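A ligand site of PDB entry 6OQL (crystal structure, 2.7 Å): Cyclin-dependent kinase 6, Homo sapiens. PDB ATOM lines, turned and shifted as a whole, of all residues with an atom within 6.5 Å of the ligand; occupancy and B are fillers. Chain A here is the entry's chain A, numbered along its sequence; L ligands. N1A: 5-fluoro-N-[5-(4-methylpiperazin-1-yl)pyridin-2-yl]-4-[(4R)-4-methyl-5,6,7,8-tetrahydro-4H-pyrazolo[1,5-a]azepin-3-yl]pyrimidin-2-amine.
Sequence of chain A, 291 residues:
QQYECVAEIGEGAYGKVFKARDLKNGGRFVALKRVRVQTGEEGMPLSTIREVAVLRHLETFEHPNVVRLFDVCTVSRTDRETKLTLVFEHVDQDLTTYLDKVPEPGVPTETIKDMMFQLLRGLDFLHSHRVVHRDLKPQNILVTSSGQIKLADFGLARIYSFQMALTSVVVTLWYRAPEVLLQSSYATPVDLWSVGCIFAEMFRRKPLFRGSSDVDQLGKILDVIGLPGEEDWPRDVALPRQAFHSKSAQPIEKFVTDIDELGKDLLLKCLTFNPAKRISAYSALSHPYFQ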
ATOM      1  N   GLU A   8       6.103  -8.095 -22.054  1.00  0.00           N
ATOM      2  CA  GLU A   8       7.453  -8.117 -21.505  1.00  0.00           C
ATOM      3  C   GLU A   8       7.380  -8.373 -20.003  1.00  0.00           C
ATOM      4  O   GLU A   8       6.624  -7.719 -19.279  1.00  0.00           O
ATOM      5  CB  GLU A   8       8.164  -6.789 -21.773  1.00  0.00           C
ATOM      6  CG  GLU A   8       9.538  -6.693 -21.148  1.00  0.00           C
ATOM      7  CD  GLU A   8      10.089  -5.279 -21.160  1.00  0.00           C
ATOM      8  OE1 GLU A   8       9.609  -4.461 -21.966  1.00  0.00           O
ATOM      9  OE2 GLU A   8      11.002  -4.985 -20.347  1.00  0.00           O
ATOM     10  N   ILE A   9       8.179  -9.323 -19.528  1.00  0.00           N
ATOM     11  CA  ILE A   9       8.266  -9.652 -18.116  1.00  0.00           C
ATOM     12  C   ILE A   9       9.640  -9.407 -17.526  1.00  0.00           C
ATOM     13  O   ILE A   9       9.821  -9.553 -16.313  1.00  0.00           O
ATOM     14  CB  ILE A   9       7.826 -11.104 -17.835  1.00  0.00           C
ATOM     15  CG1 ILE A   9       8.697 -12.076 -18.639  1.00  0.00           C
ATOM     16  CG2 ILE A   9       6.356 -11.297 -18.170  1.00  0.00           C
ATOM     17  CD1 ILE A   9       8.414 -13.522 -18.345  1.00  0.00           C
ATOM     18  N   GLY A  10      10.632  -9.041 -18.340  1.00  0.00           N
ATOM     19  CA  GLY A  10      11.964  -8.806 -17.836  1.00  0.00           C
ATOM     20  C   GLY A  10      12.899  -8.159 -18.833  1.00  0.00           C
ATOM     21  O   GLY A  10      12.865  -8.455 -20.029  1.00  0.00           O
ATOM     22  N   GLU A  11      13.762  -7.268 -18.344  1.00  0.00           N
ATOM     23  CA  GLU A  11      14.745  -6.573 -19.174  1.00  0.00           C
ATOM     24  C   GLU A  11      16.004  -6.394 -18.342  1.00  0.00           C
ATOM     25  O   GLU A  11      15.943  -6.255 -17.123  1.00  0.00           O
ATOM     26  CB  GLU A  11      14.205  -5.215 -19.660  1.00  0.00           C
ATOM     27  CG  GLU A  11      15.220  -4.332 -20.394  1.00  0.00           C
ATOM     28  CD  GLU A  11      15.232  -4.562 -21.905  1.00  0.00           C
ATOM     29  OE1 GLU A  11      14.597  -3.773 -22.633  1.00  0.00           O
ATOM     30  OE2 GLU A  11      15.870  -5.538 -22.349  1.00  0.00           O
ATOM     31  N   TYR A  14      21.065  -9.341 -19.097  1.00  0.00           N
ATOM     32  CA  TYR A  14      20.959 -10.730 -19.541  1.00  0.00           C
ATOM     33  C   TYR A  14      20.228 -10.860 -20.870  1.00  0.00           C
ATOM     34  O   TYR A  14      20.401 -11.864 -21.566  1.00  0.00           O
ATOM     35  CB  TYR A  14      20.237 -11.556 -18.472  1.00  0.00           C
ATOM     36  CG  TYR A  14      18.960 -10.913 -17.984  1.00  0.00           C
ATOM     37  CD1 TYR A  14      17.766 -11.096 -18.666  1.00  0.00           C
ATOM     38  CD2 TYR A  14      18.941 -10.103 -16.853  1.00  0.00           C
ATOM     39  CE1 TYR A  14      16.595 -10.504 -18.234  1.00  0.00           C
ATOM     40  CE2 TYR A  14      17.773  -9.498 -16.414  1.00  0.00           C
ATOM     41  CZ  TYR A  14      16.602  -9.713 -17.112  1.00  0.00           C
ATOM     42  OH  TYR A  14      15.430  -9.123 -16.689  1.00  0.00           O
ATOM     43  N   GLY A  15      19.420  -9.868 -21.229  1.00  0.00           N
ATOM     44  CA  GLY A  15      18.581  -9.947 -22.408  1.00  0.00           C
ATOM     45  C   GLY A  15      17.174  -9.480 -22.098  1.00  0.00           C
ATOM     46  O   GLY A  15      16.880  -9.099 -20.966  1.00  0.00           O
ATOM     47  N   VAL A  17      13.258 -10.493 -21.801  1.00  0.00           N
ATOM     48  CA  VAL A  17      12.440 -11.680 -21.590  1.00  0.00           C
ATOM     49  C   VAL A  17      10.985 -11.328 -21.894  1.00  0.00           C
ATOM     50  O   VAL A  17      10.507 -10.237 -21.555  1.00  0.00           O
ATOM     51  CB  VAL A  17      12.594 -12.219 -20.156  1.00  0.00           C
ATOM     52  CG1 VAL A  17      11.845 -13.532 -19.993  1.00  0.00           C
ATOM     53  CG2 VAL A  17      14.060 -12.402 -19.821  1.00  0.00           C
ATOM     54  N   PHE A  18      10.283 -12.253 -22.548  1.00  0.00           N
ATOM     55  CA  PHE A  18       8.897 -12.060 -22.932  1.00  0.00           C
ATOM     56  C   PHE A  18       8.039 -13.220 -22.447  1.00  0.00           C
ATOM     57  O   PHE A  18       8.512 -14.357 -22.325  1.00  0.00           O
ATOM     58  CB  PHE A  18       8.743 -11.927 -24.453  1.00  0.00           C
ATOM     59  CG  PHE A  18       9.188 -10.608 -24.990  1.00  0.00           C
ATOM     60  CD1 PHE A  18      10.507 -10.409 -25.352  1.00  0.00           C
ATOM     61  CD2 PHE A  18       8.287  -9.571 -25.145  1.00  0.00           C
ATOM     62  CE1 PHE A  18      10.931  -9.195 -25.864  1.00  0.00           C
ATOM     63  CE2 PHE A  18       8.702  -8.354 -25.656  1.00  0.00           C
ATOM     64  CZ  PHE A  18      10.018  -8.165 -26.015  1.00  0.00           C
ATOM     65  N   LYS A  19       6.778 -12.916 -22.154  1.00  0.00           N
ATOM     66  CA  LYS A  19       5.753 -13.923 -21.943  1.00  0.00           C
ATOM     67  C   LYS A  19       5.083 -14.187 -23.284  1.00  0.00           C
ATOM     68  O   LYS A  19       4.657 -13.235 -23.950  1.00  0.00           O
ATOM     69  CB  LYS A  19       4.740 -13.452 -20.896  1.00  0.00           C
ATOM     70  CG  LYS A  19       3.778 -14.533 -20.396  1.00  0.00           C
ATOM     71  CD  LYS A  19       2.690 -13.900 -19.546  1.00  0.00           C
ATOM     72  CE  LYS A  19       1.777 -14.953 -18.936  1.00  0.00           C
ATOM     73  NZ  LYS A  19       0.595 -14.344 -18.242  1.00  0.00           N
ATOM     74  N   VAL A  30       4.930 -19.420 -22.266  1.00  0.00           N
ATOM     75  CA  VAL A  30       6.361 -19.722 -22.207  1.00  0.00           C
ATOM     76  C   VAL A  30       7.112 -18.408 -22.053  1.00  0.00           C
ATOM     77  O   VAL A  30       6.569 -17.324 -22.241  1.00  0.00           O
ATOM     78  CB  VAL A  30       6.854 -20.483 -23.456  1.00  0.00           C
ATOM     79  CG1 VAL A  30       6.153 -21.819 -23.581  1.00  0.00           C
ATOM     80  CG2 VAL A  30       6.646 -19.633 -24.702  1.00  0.00           C
ATOM     81  N   ALA A  31       8.390 -18.525 -21.695  1.00  0.00           N
ATOM     82  CA  ALA A  31       9.264 -17.375 -21.480  1.00  0.00           C
ATOM     83  C   ALA A  31      10.303 -17.339 -22.603  1.00  0.00           C
ATOM     84  O   ALA A  31      11.178 -18.206 -22.687  1.00  0.00           O
ATOM     85  CB  ALA A  31       9.940 -17.449 -20.120  1.00  0.00           C
ATOM     86  N   LYS A  33      13.475 -15.426 -24.652  1.00  0.00           N
ATOM     87  CA  LYS A  33      14.658 -14.655 -24.298  1.00  0.00           C
ATOM     88  C   LYS A  33      15.615 -14.679 -25.484  1.00  0.00           C
ATOM     89  O   LYS A  33      15.858 -15.749 -26.054  1.00  0.00           O
ATOM     90  CB  LYS A  33      15.328 -15.205 -23.044  1.00  0.00           C
ATOM     91  CG  LYS A  33      16.553 -14.427 -22.583  1.00  0.00           C
ATOM     92  CD  LYS A  33      17.333 -15.150 -21.487  1.00  0.00           C
ATOM     93  CE  LYS A  33      16.723 -14.955 -20.105  1.00  0.00           C
ATOM     94  NZ  LYS A  33      17.538 -15.598 -19.039  1.00  0.00           N
ATOM     95  N   VAL A  67      14.304 -23.821 -14.043  1.00  0.00           N
ATOM     96  CA  VAL A  67      13.286 -23.585 -15.065  1.00  0.00           C
ATOM     97  C   VAL A  67      13.607 -24.433 -16.290  1.00  0.00           C
ATOM     98  O   VAL A  67      14.760 -24.518 -16.727  1.00  0.00           O
ATOM     99  CB  VAL A  67      13.197 -22.086 -15.386  1.00  0.00           C
ATOM    100  CG1 VAL A  67      14.381 -21.599 -16.206  1.00  0.00           C
ATOM    101  CG2 VAL A  67      11.896 -21.758 -16.048  1.00  0.00           C
ATOM    102  N   ARG A  68      12.592 -25.121 -16.805  1.00  0.00           N
ATOM    103  CA  ARG A  68      12.800 -26.072 -17.894  1.00  0.00           C
ATOM    104  C   ARG A  68      12.987 -25.348 -19.221  1.00  0.00           C
ATOM    105  O   ARG A  68      12.336 -24.337 -19.496  1.00  0.00           O
ATOM    106  CB  ARG A  68      11.611 -27.032 -17.986  1.00  0.00           C
ATOM    107  N   PHE A  88      11.652 -21.055 -22.323  1.00  0.00           N
ATOM    108  CA  PHE A  88      11.577 -21.687 -21.011  1.00  0.00           C
ATOM    109  C   PHE A  88      10.125 -21.894 -20.623  1.00  0.00           C
ATOM    110  O   PHE A  88       9.209 -21.346 -21.240  1.00  0.00           O
ATOM    111  CB  PHE A  88      12.292 -20.838 -19.944  1.00  0.00           C
ATOM    112  CG  PHE A  88      13.737 -20.567 -20.244  1.00  0.00           C
ATOM    113  CD1 PHE A  88      14.708 -21.506 -19.919  1.00  0.00           C
ATOM    114  CD2 PHE A  88      14.120 -19.366 -20.819  1.00  0.00           C
ATOM    115  CE1 PHE A  88      16.037 -21.258 -20.193  1.00  0.00           C
ATOM    116  CE2 PHE A  88      15.449 -19.118 -21.092  1.00  0.00           C
ATOM    117  CZ  PHE A  88      16.409 -20.058 -20.776  1.00  0.00           C
ATOM    118  N   GLU A  89       9.920 -22.702 -19.585  1.00  0.00           N
ATOM    119  CA  GLU A  89       8.583 -22.847 -19.014  1.00  0.00           C
ATOM    120  C   GLU A  89       8.239 -21.583 -18.253  1.00  0.00           C
ATOM    121  O   GLU A  89       8.985 -21.147 -17.370  1.00  0.00           O
ATOM    122  CB  GLU A  89       8.515 -24.080 -18.101  1.00  0.00           C
ATOM    123  CG  GLU A  89       9.470 -24.076 -16.919  1.00  0.00           C
ATOM    124  CD  GLU A  89       9.175 -25.175 -15.903  1.00  0.00           C
ATOM    125  OE1 GLU A  89      10.132 -25.864 -15.484  1.00  0.00           O
ATOM    126  OE2 GLU A  89       7.997 -25.348 -15.541  1.00  0.00           O
ATOM    127  N   HIS A  90       7.122 -20.949 -18.607  1.00  0.00           N
ATOM    128  CA  HIS A  90       6.695 -19.760 -17.893  1.00  0.00           C
ATOM    129  C   HIS A  90       6.136 -20.142 -16.533  1.00  0.00           C
ATOM    130  O   HIS A  90       5.230 -20.985 -16.435  1.00  0.00           O
ATOM    131  CB  HIS A  90       5.651 -18.976 -18.677  1.00  0.00           C
ATOM    132  CG  HIS A  90       5.087 -17.814 -17.931  1.00  0.00           C
ATOM    133  ND1 HIS A  90       5.799 -16.647 -17.725  1.00  0.00           N
ATOM    134  CD2 HIS A  90       3.890 -17.638 -17.314  1.00  0.00           C
ATOM    135  CE1 HIS A  90       5.063 -15.803 -17.032  1.00  0.00           C
ATOM    136  NE2 HIS A  90       3.906 -16.377 -16.762  1.00  0.00           N
ATOM    137  N   VAL A  91       6.679 -19.535 -15.488  1.00  0.00           N
ATOM    138  CA  VAL A  91       6.159 -19.657 -14.131  1.00  0.00           C
ATOM    139  C   VAL A  91       5.630 -18.284 -13.722  1.00  0.00           C
ATOM    140  O   VAL A  91       6.309 -17.273 -13.896  1.00  0.00           O
ATOM    141  CB  VAL A  91       7.237 -20.159 -13.132  1.00  0.00           C
ATOM    142  CG1 VAL A  91       8.625 -19.965 -13.717  1.00  0.00           C
ATOM    143  CG2 VAL A  91       7.115 -19.441 -11.795  1.00  0.00           C
ATOM    144  N   ASP A  92       4.427 -18.288 -13.164  1.00  0.00           N
ATOM    145  CA  ASP A  92       3.546 -17.115 -13.131  1.00  0.00           C
ATOM    146  C   ASP A  92       4.154 -15.905 -12.421  1.00  0.00           C
ATOM    147  O   ASP A  92       3.822 -14.769 -12.779  1.00  0.00           O
ATOM    148  CB  ASP A  92       2.220 -17.508 -12.495  1.00  0.00           C
ATOM    149  CG  ASP A  92       1.535 -18.633 -13.249  1.00  0.00           C
ATOM    150  OD1 ASP A  92       0.607 -18.339 -14.018  1.00  0.00           O
ATOM    151  OD2 ASP A  92       1.963 -19.795 -13.101  1.00  0.00           O
ATOM    152  N   GLN A  93       5.020 -16.112 -11.435  1.00  0.00           N
ATOM    153  CA  GLN A  93       5.545 -14.961 -10.693  1.00  0.00           C
ATOM    154  C   GLN A  93       6.918 -15.300 -10.113  1.00  0.00           C
ATOM    155  O   GLN A  93       7.289 -16.471  -9.995  1.00  0.00           O
ATOM    156  CB  GLN A  93       4.595 -14.514  -9.586  1.00  0.00           C
ATOM    157  CG  GLN A  93       4.345 -15.598  -8.561  1.00  0.00           C
ATOM    158  CD  GLN A  93       3.916 -15.052  -7.213  1.00  0.00           C
ATOM    159  OE1 GLN A  93       4.074 -15.710  -6.188  1.00  0.00           O
ATOM    160  NE2 GLN A  93       3.383 -13.829  -7.213  1.00  0.00           N
ATOM    161  N   ASP A  94       7.659 -14.255  -9.747  1.00  0.00           N
ATOM    162  CA  ASP A  94       8.981 -14.410  -9.163  1.00  0.00           C
ATOM    163  C   ASP A  94       8.902 -14.252  -7.649  1.00  0.00           C
ATOM    164  O   ASP A  94       7.839 -14.018  -7.072  1.00  0.00           O
ATOM    165  CB  ASP A  94       9.968 -13.432  -9.794  1.00  0.00           C
ATOM    166  CG  ASP A  94       9.666 -11.979  -9.459  1.00  0.00           C
ATOM    167  OD1 ASP A  94       8.608 -11.685  -8.859  1.00  0.00           O
ATOM    168  OD2 ASP A  94      10.510 -11.120  -9.795  1.00  0.00           O
ATOM    169  N   THR A  96      10.208 -11.822  -5.867  1.00  0.00           N
ATOM    170  CA  THR A  96      10.065 -10.447  -5.419  1.00  0.00           C
ATOM    171  C   THR A  96       8.598 -10.016  -5.406  1.00  0.00           C
ATOM    172  O   THR A  96       8.213  -9.184  -4.579  1.00  0.00           O
ATOM    173  CB  THR A  96      10.914  -9.514  -6.288  1.00  0.00           C
ATOM    174  OG1 THR A  96      11.632  -8.594  -5.455  1.00  0.00           O
ATOM    175  CG2 THR A  96      10.058  -8.718  -7.278  1.00  0.00           C
ATOM    176  N   THR A  97       7.775 -10.558  -6.296  1.00  0.00           N
ATOM    177  CA  THR A  97       6.346 -10.281  -6.273  1.00  0.00           C
ATOM    178  C   THR A  97       5.582 -11.257  -5.384  1.00  0.00           C
ATOM    179  O   THR A  97       4.430 -10.991  -5.046  1.00  0.00           O
ATOM    180  CB  THR A  97       5.763 -10.310  -7.692  1.00  0.00           C
ATOM    181  OG1 THR A  97       6.255 -11.451  -8.389  1.00  0.00           O
ATOM    182  CG2 THR A  97       6.133  -9.048  -8.442  1.00  0.00           C
ATOM    183  N   LYS A 137      19.445 -13.819  -7.051  1.00  0.00           N
ATOM    184  CA  LYS A 137      18.693 -12.748  -6.425  1.00  0.00           C
ATOM    185  C   LYS A 137      17.205 -13.062  -6.560  1.00  0.00           C
ATOM    186  O   LYS A 137      16.820 -13.938  -7.358  1.00  0.00           O
ATOM    187  CB  LYS A 137      19.036 -11.386  -7.053  1.00  0.00           C
ATOM    188  CG  LYS A 137      18.217 -11.044  -8.280  1.00  0.00           C
ATOM    189  CD  LYS A 137      19.023 -10.172  -9.229  1.00  0.00           C
ATOM    190  CE  LYS A 137      18.348 -10.088 -10.592  1.00  0.00           C
ATOM    191  NZ  LYS A 137      19.246  -9.462 -11.609  1.00  0.00           N
ATOM    192  N   GLN A 139      14.811 -11.692  -8.067  1.00  0.00           N
ATOM    193  CA  GLN A 139      14.218 -11.535  -9.393  1.00  0.00           C
ATOM    194  C   GLN A 139      14.447 -12.753 -10.275  1.00  0.00           C
ATOM    195  O   GLN A 139      13.683 -12.971 -11.222  1.00  0.00           O
ATOM    196  CB  GLN A 139      14.749 -10.278 -10.063  1.00  0.00           C
ATOM    197  CG  GLN A 139      14.175  -8.985  -9.505  1.00  0.00           C
ATOM    198  CD  GLN A 139      14.780  -8.596  -8.181  1.00  0.00           C
ATOM    199  OE1 GLN A 139      16.001  -8.655  -8.001  1.00  0.00           O
ATOM    200  NE2 GLN A 139      13.946  -8.202  -7.226  1.00  0.00           N
ATOM    201  N   ASN A 140      15.475 -13.559 -10.001  1.00  0.00           N
ATOM    202  CA  ASN A 140      15.681 -14.794 -10.758  1.00  0.00           C
ATOM    203  C   ASN A 140      15.015 -15.995 -10.124  1.00  0.00           C
ATOM    204  O   ASN A 140      14.846 -17.026 -10.784  1.00  0.00           O
ATOM    205  CB  ASN A 140      17.176 -15.093 -10.902  1.00  0.00           C
ATOM    206  CG  ASN A 140      18.000 -13.839 -11.007  1.00  0.00           C
ATOM    207  OD1 ASN A 140      18.661 -13.448 -10.053  1.00  0.00           O
ATOM    208  ND2 ASN A 140      17.961 -13.186 -12.167  1.00  0.00           N
ATOM    209  N   LEU A 142      11.944 -17.952  -9.023  1.00  0.00           N
ATOM    210  CA  LEU A 142      10.562 -17.977  -9.478  1.00  0.00           C
ATOM    211  C   LEU A 142       9.748 -18.964  -8.651  1.00  0.00           C
ATOM    212  O   LEU A 142      10.273 -19.981  -8.183  1.00  0.00           O
ATOM    213  CB  LEU A 142      10.501 -18.356 -10.962  1.00  0.00           C
ATOM    214  CG  LEU A 142      11.497 -17.589 -11.827  1.00  0.00           C
ATOM    215  CD1 LEU A 142      11.600 -18.193 -13.217  1.00  0.00           C
ATOM    216  CD2 LEU A 142      11.115 -16.122 -11.907  1.00  0.00           C
ATOM    217  N   LEU A 151      14.734 -21.993 -10.471  1.00  0.00           N
ATOM    218  CA  LEU A 151      15.794 -21.034 -10.737  1.00  0.00           C
ATOM    219  C   LEU A 151      15.857 -20.694 -12.221  1.00  0.00           C
ATOM    220  O   LEU A 151      15.585 -21.541 -13.090  1.00  0.00           O
ATOM    221  CB  LEU A 151      17.157 -21.578 -10.294  1.00  0.00           C
ATOM    222  CG  LEU A 151      17.273 -21.907  -8.802  1.00  0.00           C
ATOM    223  CD1 LEU A 151      18.656 -22.476  -8.514  1.00  0.00           C
ATOM    224  CD2 LEU A 151      17.003 -20.673  -7.960  1.00  0.00           C
ATOM    225  N   ALA A 152      16.238 -19.450 -12.512  1.00  0.00           N
ATOM    226  CA  ALA A 152      16.364 -18.975 -13.879  1.00  0.00           C
ATOM    227  C   ALA A 152      17.557 -18.049 -13.978  1.00  0.00           C
ATOM    228  O   ALA A 152      18.176 -17.684 -12.967  1.00  0.00           O
ATOM    229  CB  ALA A 152      15.099 -18.258 -14.361  1.00  0.00           C
ATOM    230  N   ASP A 153      17.881 -17.665 -15.213  1.00  0.00           N
ATOM    231  CA  ASP A 153      18.918 -16.665 -15.499  1.00  0.00           C
ATOM    232  C   ASP A 153      20.293 -17.131 -15.008  1.00  0.00           C
ATOM    233  O   ASP A 153      20.923 -16.519 -14.150  1.00  0.00           O
ATOM    234  CB  ASP A 153      18.538 -15.310 -14.898  1.00  0.00           C
ATOM    235  CG  ASP A 153      19.040 -14.147 -15.736  1.00  0.00           C
ATOM    236  OD1 ASP A 153      18.689 -14.078 -16.928  1.00  0.00           O
ATOM    237  OD2 ASP A 153      19.766 -13.296 -15.191  1.00  0.00           O
HETATM  238  C4  N1A L   1      15.412 -12.470 -14.952  1.00  0.00           C
HETATM  239  C5  N1A L   1      15.322 -13.059 -16.345  1.00  0.00           C
HETATM  240  C6  N1A L   1      13.148 -14.372 -16.086  1.00  0.00           C
HETATM  241  N1  N1A L   1      14.962 -15.377 -16.978  1.00  0.00           N
HETATM  242  C7  N1A L   1      12.794 -15.681 -16.405  1.00  0.00           C
HETATM  243  C8  N1A L   1      13.962 -16.237 -16.954  1.00  0.00           C
HETATM  244  N2  N1A L   1       8.977 -17.509 -16.138  1.00  0.00           N
HETATM  245  C9  N1A L   1      11.504 -16.361 -16.302  1.00  0.00           C
HETATM  246  C10 N1A L   1      11.253 -17.684 -16.794  1.00  0.00           C
HETATM  247  C11 N1A L   1       9.993 -18.193 -16.675  1.00  0.00           C
HETATM  248  C12 N1A L   1       9.284 -16.286 -15.689  1.00  0.00           C
HETATM  249  N3  N1A L   1      10.489 -15.687 -15.731  1.00  0.00           N
HETATM  250  C13 N1A L   1       8.048 -14.295 -14.692  1.00  0.00           C
HETATM  251  C14 N1A L   1       9.108 -13.543 -14.183  1.00  0.00           C
HETATM  252  C15 N1A L   1       8.849 -12.265 -13.738  1.00  0.00           C
HETATM  253  N4  N1A L   1       8.220 -15.537 -15.270  1.00  0.00           N
HETATM  254  N   N1A L   1      14.456 -14.223 -16.441  1.00  0.00           N
HETATM  255  C   N1A L   1      11.880 -12.286 -16.555  1.00  0.00           C
HETATM  256  C1  N1A L   1      12.315 -13.283 -15.483  1.00  0.00           C
HETATM  257  C16 N1A L   1       7.558 -11.748 -13.814  1.00  0.00           C
HETATM  258  C17 N1A L   1       6.563 -12.576 -14.320  1.00  0.00           C
HETATM  259  C18 N1A L   1       6.522  -9.578 -14.317  1.00  0.00           C
HETATM  260  C19 N1A L   1       6.843  -8.126 -14.036  1.00  0.00           C
HETATM  261  C2  N1A L   1      12.942 -12.626 -14.245  1.00  0.00           C
HETATM  262  C20 N1A L   1       7.392  -8.661 -11.770  1.00  0.00           C
HETATM  263  C21 N1A L   1       7.072 -10.123 -12.016  1.00  0.00           C
HETATM  264  C22 N1A L   1       6.874  -6.390 -12.372  1.00  0.00           C
HETATM  265  C3  N1A L   1      14.173 -11.749 -14.463  1.00  0.00           C
HETATM  266  F   N1A L   1      12.217 -18.437 -17.374  1.00  0.00           F
HETATM  267  N5  N1A L   1       6.790 -13.821 -14.749  1.00  0.00           N
HETATM  268  N6  N1A L   1       7.286 -10.454 -13.425  1.00  0.00           N
HETATM  269  N7  N1A L   1       6.586  -7.798 -12.630  1.00  0.00           N
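N of Val 91 is in hydrogen-bond range of N2 of the ligand (3.1 Å).
O of Val 91 lies close to N4 of the ligand (2.9 Å).
The side-chain amino group of Lys 33 is in hydrogen-bond range of a nitrogen (N1) of the ligand, 3.3 Å away.
The side-chain amide nitrogen of Gln 139 lies within hydrogen-bond range of the side-chain hydroxyl of Thr 96, 2.9 Å away.
OE1 of Glu 89 lies within hydrogen-bond range of N of Arg 68 (2.9 Å).
The side-chain amino group of Lys 33 lies within salt-bridge range of the side-chain carboxylate of Asp 153, at 2.8 Å.
The backbone carbonyl oxygen (O) of Asn 140 is in hydrogen-bond range of the backbone NH (N) of Ala 152.
The backbone NH of Phe 88 sits at hydrogen-bond distance from the backbone carbonyl oxygen of Ala 31 (2.9 Å).
The side-chain hydroxyl (OG1) of Thr 97 sits at hydrogen-bond distance from the side-chain carboxylate (OD1) of Asp 94 (2.4 Å).
The backbone NH (N) of Thr 96 lies close to the side-chain carboxylate (OD1) of Asp 94.
The backbone NH (N) of Lys 137 lies close to the side-chain amide oxygen (OD1) of Asn 140 (3.1 Å).
Ile 9 touches the ligand.
Gly 10 touches the ligand (CA to C, 3.7 Å).
CE1 of Tyr 14 touches C5 of the ligand (3.4 Å).
CG1 of Val 17 touches C of the ligand, at 3.7 Å.
CB of Ala 31 touches C11 of the ligand, at 3.5 Å.
CG2 of Val 67 touches F of the ligand (3.6 Å).
Phe 88 touches the ligand (CB to F, 3.5 Å).
Glu 89 touches the ligand.
His 90 touches the ligand (CE1 to N5, 3.5 Å).
Asp 92 touches the ligand.
Asp 94 touches the ligand (OD1 to C21, 3.8 Å).
Thr 97 touches the ligand.
Gln 139 touches the ligand (O to C2, 3.1 Å).
ND2 of Asn 140 touches C4 of the ligand (3.8 Å).
Leu 142 touches the ligand.
CB of Ala 152 touches C8 of the ligand, 3.5 Å away.
Asp 153 touches the ligand (OD1 to C5, 3.6 Å).
Hydrophobic or aromatic side chains that line the ligand: Ile 9, Tyr 14, Val 17, Ala 31, Val 67, Phe 88, His 90, Val 91, Leu 142 and Ala 152.
Of the 30 residues printed, 19 come within 4 Å of the ligand.
The nearest printed residue that does not touch the ligand is Gln 93 (4.4 Å).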
